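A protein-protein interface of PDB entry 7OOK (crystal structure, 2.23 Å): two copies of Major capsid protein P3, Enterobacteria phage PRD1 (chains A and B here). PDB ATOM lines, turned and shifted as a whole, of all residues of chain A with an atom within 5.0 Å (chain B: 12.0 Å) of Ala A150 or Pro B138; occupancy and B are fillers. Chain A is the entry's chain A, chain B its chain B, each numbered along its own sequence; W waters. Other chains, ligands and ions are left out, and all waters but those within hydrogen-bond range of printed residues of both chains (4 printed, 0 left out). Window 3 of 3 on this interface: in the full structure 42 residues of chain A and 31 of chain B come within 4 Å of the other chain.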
ATOM      1  N   LEU A  87      23.471  25.607  24.380  1.00  0.00           N
ATOM      2  CA  LEU A  87      22.573  25.127  25.419  1.00  0.00           C
ATOM      3  C   LEU A  87      22.716  23.626  25.627  1.00  0.00           C
ATOM      4  O   LEU A  87      22.867  22.860  24.674  1.00  0.00           O
ATOM      5  CB  LEU A  87      21.124  25.437  25.052  1.00  0.00           C
ATOM      6  CG  LEU A  87      20.577  26.825  25.352  1.00  0.00           C
ATOM      7  CD1 LEU A  87      19.191  26.930  24.733  1.00  0.00           C
ATOM      8  CD2 LEU A  87      20.529  27.088  26.847  1.00  0.00           C
ATOM      9  N   ASP A  89      20.786  20.088  27.193  1.00  0.00           N
ATOM     10  CA  ASP A  89      19.435  19.584  26.971  1.00  0.00           C
ATOM     11  C   ASP A  89      18.426  20.269  27.886  1.00  0.00           C
ATOM     12  O   ASP A  89      17.292  20.538  27.474  1.00  0.00           O
ATOM     13  CB  ASP A  89      19.403  18.068  27.168  1.00  0.00           C
ATOM     14  CG  ASP A  89      19.973  17.308  25.979  1.00  0.00           C
ATOM     15  OD1 ASP A  89      20.270  17.944  24.944  1.00  0.00           O
ATOM     16  OD2 ASP A  89      20.123  16.070  26.081  1.00  0.00           O
ATOM     17  N   PRO A  92      17.861  26.519  30.284  1.00  0.00           N
ATOM     18  CA  PRO A  92      17.447  27.447  31.353  1.00  0.00           C
ATOM     19  C   PRO A  92      16.694  26.783  32.491  1.00  0.00           C
ATOM     20  O   PRO A  92      16.476  27.438  33.521  1.00  0.00           O
ATOM     21  CB  PRO A  92      16.554  28.458  30.619  1.00  0.00           C
ATOM     22  CG  PRO A  92      16.011  27.700  29.462  1.00  0.00           C
ATOM     23  CD  PRO A  92      17.110  26.758  29.035  1.00  0.00           C
ATOM     24  N   ILE A 148       9.541  31.884  28.330  1.00  0.00           N
ATOM     25  CA  ILE A 148      10.685  31.036  28.651  1.00  0.00           C
ATOM     26  C   ILE A 148      11.587  31.038  27.427  1.00  0.00           C
ATOM     27  O   ILE A 148      11.180  30.590  26.348  1.00  0.00           O
ATOM     28  CB  ILE A 148      10.264  29.612  29.045  1.00  0.00           C
ATOM     29  CG1 ILE A 148       9.457  29.667  30.347  1.00  0.00           C
ATOM     30  CG2 ILE A 148      11.489  28.715  29.197  1.00  0.00           C
ATOM     31  CD1 ILE A 148       9.053  28.318  30.900  1.00  0.00           C
ATOM     32  N   ASP A 149      12.806  31.543  27.593  1.00  0.00           N
ATOM     33  CA  ASP A 149      13.642  31.888  26.455  1.00  0.00           C
ATOM     34  C   ASP A 149      15.111  31.821  26.841  1.00  0.00           C
ATOM     35  O   ASP A 149      15.484  32.154  27.969  1.00  0.00           O
ATOM     36  CB  ASP A 149      13.291  33.292  25.946  1.00  0.00           C
ATOM     37  CG  ASP A 149      14.152  33.726  24.782  1.00  0.00           C
ATOM     38  OD1 ASP A 149      14.025  33.127  23.695  1.00  0.00           O
ATOM     39  OD2 ASP A 149      14.949  34.673  24.953  1.00  0.00           O
ATOM     40  N   ALA A 150      15.936  31.388  25.890  1.00  0.00           N
ATOM     41  CA  ALA A 150      17.386  31.374  26.044  1.00  0.00           C
ATOM     42  C   ALA A 150      18.031  31.194  24.676  1.00  0.00           C
ATOM     43  O   ALA A 150      17.612  30.319  23.908  1.00  0.00           O
ATOM     44  CB  ALA A 150      17.828  30.257  26.986  1.00  0.00           C
ATOM     45  N   PRO A 151      19.045  31.990  24.332  1.00  0.00           N
ATOM     46  CA  PRO A 151      19.698  31.810  23.030  1.00  0.00           C
ATOM     47  C   PRO A 151      20.316  30.425  22.910  1.00  0.00           C
ATOM     48  O   PRO A 151      20.924  29.906  23.849  1.00  0.00           O
ATOM     49  CB  PRO A 151      20.761  32.917  23.000  1.00  0.00           C
ATOM     50  CG  PRO A 151      20.942  33.339  24.413  1.00  0.00           C
ATOM     51  CD  PRO A 151      19.622  33.115  25.092  1.00  0.00           C
ATOM     52  N   ALA A 152      20.134  29.821  21.734  1.00  0.00           N
ATOM     53  CA  ALA A 152      20.669  28.487  21.498  1.00  0.00           C
ATOM     54  C   ALA A 152      22.181  28.455  21.650  1.00  0.00           C
ATOM     55  O   ALA A 152      22.742  27.435  22.070  1.00  0.00           O
ATOM     56  CB  ALA A 152      20.270  28.008  20.101  1.00  0.00           C
ATOM     57  N   GLU A 161      20.518  36.779  27.046  1.00  0.00           N
ATOM     58  CA  GLU A 161      19.489  37.000  28.055  1.00  0.00           C
ATOM     59  C   GLU A 161      18.614  35.759  28.157  1.00  0.00           C
ATOM     60  O   GLU A 161      18.160  35.229  27.136  1.00  0.00           O
ATOM     61  CB  GLU A 161      18.631  38.218  27.705  1.00  0.00           C
ATOM     62  CG  GLU A 161      19.413  39.490  27.423  1.00  0.00           C
ATOM     63  CD  GLU A 161      19.818  40.236  28.682  1.00  0.00           C
ATOM     64  OE1 GLU A 161      19.529  39.743  29.795  1.00  0.00           O
ATOM     65  OE2 GLU A 161      20.426  41.320  28.554  1.00  0.00           O
ATOM     66  N   LEU A 162      18.376  35.302  29.386  1.00  0.00           N
ATOM     67  CA  LEU A 162      17.567  34.122  29.649  1.00  0.00           C
ATOM     68  C   LEU A 162      16.371  34.494  30.515  1.00  0.00           C
ATOM     69  O   LEU A 162      16.440  35.415  31.333  1.00  0.00           O
ATOM     70  CB  LEU A 162      18.377  33.021  30.360  1.00  0.00           C
ATOM     71  CG  LEU A 162      19.538  32.359  29.621  1.00  0.00           C
ATOM     72  CD1 LEU A 162      20.741  33.282  29.506  1.00  0.00           C
ATOM     73  CD2 LEU A 162      19.932  31.066  30.327  1.00  0.00           C
ATOM     74  N   TYR A 215      24.815  25.929  29.743  1.00  0.00           N
ATOM     75  CA  TYR A 215      25.542  25.957  28.484  1.00  0.00           C
ATOM     76  C   TYR A 215      26.745  25.028  28.572  1.00  0.00           C
ATOM     77  O   TYR A 215      27.298  24.798  29.651  1.00  0.00           O
ATOM     78  CB  TYR A 215      26.005  27.381  28.127  1.00  0.00           C
ATOM     79  CG  TYR A 215      24.881  28.264  27.654  1.00  0.00           C
ATOM     80  CD1 TYR A 215      24.511  28.285  26.318  1.00  0.00           C
ATOM     81  CD2 TYR A 215      24.179  29.064  28.542  1.00  0.00           C
ATOM     82  CE1 TYR A 215      23.475  29.080  25.879  1.00  0.00           C
ATOM     83  CE2 TYR A 215      23.141  29.863  28.111  1.00  0.00           C
ATOM     84  CZ  TYR A 215      22.794  29.867  26.777  1.00  0.00           C
ATOM     85  OH  TYR A 215      21.760  30.660  26.344  1.00  0.00           O
ATOM     86  N   MET B 133       4.704  17.777  18.954  1.00  0.00           N
ATOM     87  CA  MET B 133       4.385  19.164  18.647  1.00  0.00           C
ATOM     88  C   MET B 133       5.642  20.030  18.705  1.00  0.00           C
ATOM     89  O   MET B 133       6.556  19.790  19.495  1.00  0.00           O
ATOM     90  CB  MET B 133       3.325  19.659  19.636  1.00  0.00           C
ATOM     91  CG  MET B 133       3.061  21.149  19.659  1.00  0.00           C
ATOM     92  SD  MET B 133       1.890  21.578  20.979  1.00  0.00           S
ATOM     93  CE  MET B 133       2.776  21.019  22.429  1.00  0.00           C
ATOM     94  N   VAL B 134       5.688  21.040  17.840  1.00  0.00           N
ATOM     95  CA  VAL B 134       6.809  21.971  17.771  1.00  0.00           C
ATOM     96  C   VAL B 134       6.468  23.197  18.606  1.00  0.00           C
ATOM     97  O   VAL B 134       5.368  23.755  18.482  1.00  0.00           O
ATOM     98  CB  VAL B 134       7.121  22.362  16.315  1.00  0.00           C
ATOM     99  CG1 VAL B 134       8.263  23.377  16.260  1.00  0.00           C
ATOM    100  CG2 VAL B 134       7.467  21.125  15.488  1.00  0.00           C
ATOM    101  N   THR B 135       7.400  23.616  19.464  1.00  0.00           N
ATOM    102  CA  THR B 135       7.210  24.797  20.294  1.00  0.00           C
ATOM    103  C   THR B 135       8.494  25.619  20.313  1.00  0.00           C
ATOM    104  O   THR B 135       9.540  25.196  19.811  1.00  0.00           O
ATOM    105  CB  THR B 135       6.810  24.439  21.738  1.00  0.00           C
ATOM    106  OG1 THR B 135       7.974  24.045  22.479  1.00  0.00           O
ATOM    107  CG2 THR B 135       5.791  23.309  21.766  1.00  0.00           C
ATOM    108  N   ASP B 136       8.404  26.806  20.917  1.00  0.00           N
ATOM    109  CA  ASP B 136       9.532  27.711  21.081  1.00  0.00           C
ATOM    110  C   ASP B 136      10.361  27.405  22.324  1.00  0.00           C
ATOM    111  O   ASP B 136      11.209  28.217  22.705  1.00  0.00           O
ATOM    112  CB  ASP B 136       9.037  29.159  21.170  1.00  0.00           C
ATOM    113  CG  ASP B 136       8.440  29.486  22.535  1.00  0.00           C
ATOM    114  OD1 ASP B 136       7.948  28.556  23.213  1.00  0.00           O
ATOM    115  OD2 ASP B 136       8.456  30.671  22.933  1.00  0.00           O
ATOM    116  N   SER B 137      10.121  26.278  22.974  1.00  0.00           N
ATOM    117  CA  SER B 137      10.786  26.007  24.239  1.00  0.00           C
ATOM    118  C   SER B 137      12.289  25.868  24.024  1.00  0.00           C
ATOM    119  O   SER B 137      12.719  25.094  23.155  1.00  0.00           O
ATOM    120  CB  SER B 137      10.233  24.733  24.872  1.00  0.00           C
ATOM    121  OG  SER B 137      10.848  24.500  26.125  1.00  0.00           O
ATOM    122  N   PRO B 138      13.120  26.585  24.789  1.00  0.00           N
ATOM    123  CA  PRO B 138      14.571  26.348  24.696  1.00  0.00           C
ATOM    124  C   PRO B 138      14.993  25.019  25.300  1.00  0.00           C
ATOM    125  O   PRO B 138      16.024  24.468  24.894  1.00  0.00           O
ATOM    126  CB  PRO B 138      15.173  27.537  25.457  1.00  0.00           C
ATOM    127  CG  PRO B 138      14.112  27.910  26.454  1.00  0.00           C
ATOM    128  CD  PRO B 138      12.789  27.634  25.774  1.00  0.00           C
ATOM    129  N   ILE B 139      14.240  24.495  26.271  1.00  0.00           N
ATOM    130  CA  ILE B 139      14.496  23.148  26.759  1.00  0.00           C
ATOM    131  C   ILE B 139      14.282  22.173  25.608  1.00  0.00           C
ATOM    132  O   ILE B 139      13.306  22.276  24.851  1.00  0.00           O
ATOM    133  CB  ILE B 139      13.590  22.827  27.958  1.00  0.00           C
ATOM    134  CG1 ILE B 139      13.934  23.713  29.161  1.00  0.00           C
ATOM    135  CG2 ILE B 139      13.727  21.360  28.358  1.00  0.00           C
ATOM    136  CD1 ILE B 139      13.161  25.013  29.233  1.00  0.00           C
ATOM    137  N   LYS B 140      15.198  21.217  25.463  1.00  0.00           N
ATOM    138  CA  LYS B 140      15.276  20.421  24.239  1.00  0.00           C
ATOM    139  C   LYS B 140      14.235  19.299  24.237  1.00  0.00           C
ATOM    140  O   LYS B 140      14.537  18.113  24.096  1.00  0.00           O
ATOM    141  CB  LYS B 140      16.690  19.887  24.050  1.00  0.00           C
ATOM    142  CG  LYS B 140      17.711  21.010  23.897  1.00  0.00           C
ATOM    143  CD  LYS B 140      18.908  20.607  23.053  1.00  0.00           C
ATOM    144  CE  LYS B 140      19.850  21.789  22.860  1.00  0.00           C
ATOM    145  NZ  LYS B 140      21.007  21.447  21.984  1.00  0.00           N
ATOM    146  N   TYR B 141      12.978  19.710  24.396  1.00  0.00           N
ATOM    147  CA  TYR B 141      11.862  18.875  23.995  1.00  0.00           C
ATOM    148  C   TYR B 141      11.871  18.712  22.477  1.00  0.00           C
ATOM    149  O   TYR B 141      12.596  19.401  21.753  1.00  0.00           O
ATOM    150  CB  TYR B 141      10.529  19.490  24.420  1.00  0.00           C
ATOM    151  CG  TYR B 141      10.335  19.642  25.906  1.00  0.00           C
ATOM    152  CD1 TYR B 141       9.950  18.562  26.688  1.00  0.00           C
ATOM    153  CD2 TYR B 141      10.516  20.873  26.527  1.00  0.00           C
ATOM    154  CE1 TYR B 141       9.764  18.698  28.046  1.00  0.00           C
ATOM    155  CE2 TYR B 141      10.329  21.020  27.885  1.00  0.00           C
ATOM    156  CZ  TYR B 141       9.955  19.927  28.640  1.00  0.00           C
ATOM    157  OH  TYR B 141       9.770  20.067  29.995  1.00  0.00           O
ATOM    158  N   GLY B 142      11.034  17.802  21.996  1.00  0.00           N
ATOM    159  CA  GLY B 142      10.804  17.695  20.571  1.00  0.00           C
ATOM    160  C   GLY B 142      10.811  16.268  20.080  1.00  0.00           C
ATOM    161  O   GLY B 142      10.441  15.345  20.811  1.00  0.00           O
ATOM    162  N   ASP B 143      11.224  16.083  18.828  1.00  0.00           N
ATOM    163  CA  ASP B 143      11.320  14.761  18.221  1.00  0.00           C
ATOM    164  C   ASP B 143      12.638  14.145  18.676  1.00  0.00           C
ATOM    165  O   ASP B 143      13.656  14.165  17.980  1.00  0.00           O
ATOM    166  CB  ASP B 143      11.218  14.858  16.706  1.00  0.00           C
ATOM    167  CG  ASP B 143      11.227  13.502  16.035  1.00  0.00           C
ATOM    168  OD1 ASP B 143      11.224  12.478  16.753  1.00  0.00           O
ATOM    169  OD2 ASP B 143      11.241  13.463  14.787  1.00  0.00           O
ATOM    170  N   VAL B 144      12.611  13.603  19.889  1.00  0.00           N
ATOM    171  CA  VAL B 144      13.783  12.966  20.473  1.00  0.00           C
ATOM    172  C   VAL B 144      13.819  11.480  20.151  1.00  0.00           C
ATOM    173  O   VAL B 144      14.874  10.942  19.806  1.00  0.00           O
ATOM    174  CB  VAL B 144      13.795  13.199  21.999  1.00  0.00           C
ATOM    175  CG1 VAL B 144      14.936  12.433  22.653  1.00  0.00           C
ATOM    176  CG2 VAL B 144      13.894  14.675  22.311  1.00  0.00           C
HETATM  177  O   HOH W   1       9.013  28.613  25.864  1.00  0.00           O
HETATM  178  O   HOH W   2      17.830  23.889  26.685  1.00  0.00           O
HETATM  179  O   HOH W   3      21.891  24.635  21.311  1.00  0.00           O
HETATM  180  O   HOH W   4      10.295  31.898  24.268  1.00  0.00           O
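The backbone NH (N) of Lys B140 sits at hydrogen-bond distance from the backbone carbonyl oxygen (O) of Asp A89 (3.0 Å).
The backbone NH of Leu A87 is in hydrogen-bond range of the backbone carbonyl oxygen of Ala A152 (3.0 Å).
N of Ile B139 lies close to OG of Ser B137.
Among the printed residues, pairs that only touch across the chains: Leu A87 with Lys B140, Asp A89 with Ile B139, Pro A92 with Pro B138, Pro A92 with Ile B139, Ile A148 with Pro B138 and Ala A150 with Pro B138.
Ala A150 touches just one residue of chain B: Pro B138.
Of the printed residues of chain A, Pro B138 touches Pro A92, Ile A148 and Ala A150.
Pro A92 touches just these residues of chain B: Pro B138 (3.6 Å) and Ile B139 (3.9 Å).
Ile A148 touches just one residue of chain B: Pro B138.
No residue of chain B comes within 4 Å of Pro A151.
No residue of chain B comes within 4 Å of Ala A152.
No residue of chain B comes within 4 Å of Leu A162.
Printed residues of chain A within 4 Å of Lys B140: Leu A87 (3.6 Å) and Asp A89 (3.0 Å).
Of the printed residues of chain A, Ile B139 touches Asp A89 and Pro A92.
Ser B137 touches none of the printed residues of chain A.
Gly B142 touches none of the printed residues of chain A.
Of the 11 printed residues of chain A, 5 touch a printed residue of chain B.
Hydrophobic or aromatic side chains of chain A within 4 Å of the printed part of chain B: Pro A92 and Ile A148.
Of the 12 printed residues of chain B, 3 touch a printed residue of chain A.
Printed residues of chain B that touch a printed residue of chain A: Pro B138, Ile B139 and Lys B140.
Hydrophobic or aromatic side chains of chain B that line the printed part of chain A: Pro B138 and Ile B139.
Among the printed residues, 7 pairs touch across the chains.
Among the printed residues, no Asp or Glu carboxylate lies within 4 Å of a Lys or Arg side-chain nitrogen of the other chain.
No position is printed for both chains.
Of the 7 pairs that touch across the chains among the printed residues, none has its exchanged pair printed and touching as well.
Water W4 bridges OD2 of Asp B136 (2.6 Å) and O of Ile A148 (2.6 Å).
Water W2 bridges the backbone carbonyl oxygen of Pro B138 (2.6 Å) and the backbone carbonyl oxygen of Asp A89 (3.5 Å).
Water W1 lies within hydrogen-bond range of the side-chain carboxylate of Asp B136 and the backbone carbonyl oxygen of Ile A148.
Water W3 bridges the backbone carbonyl oxygen (O) of Ala A152 and the side-chain amino group (NZ) of Lys B140.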
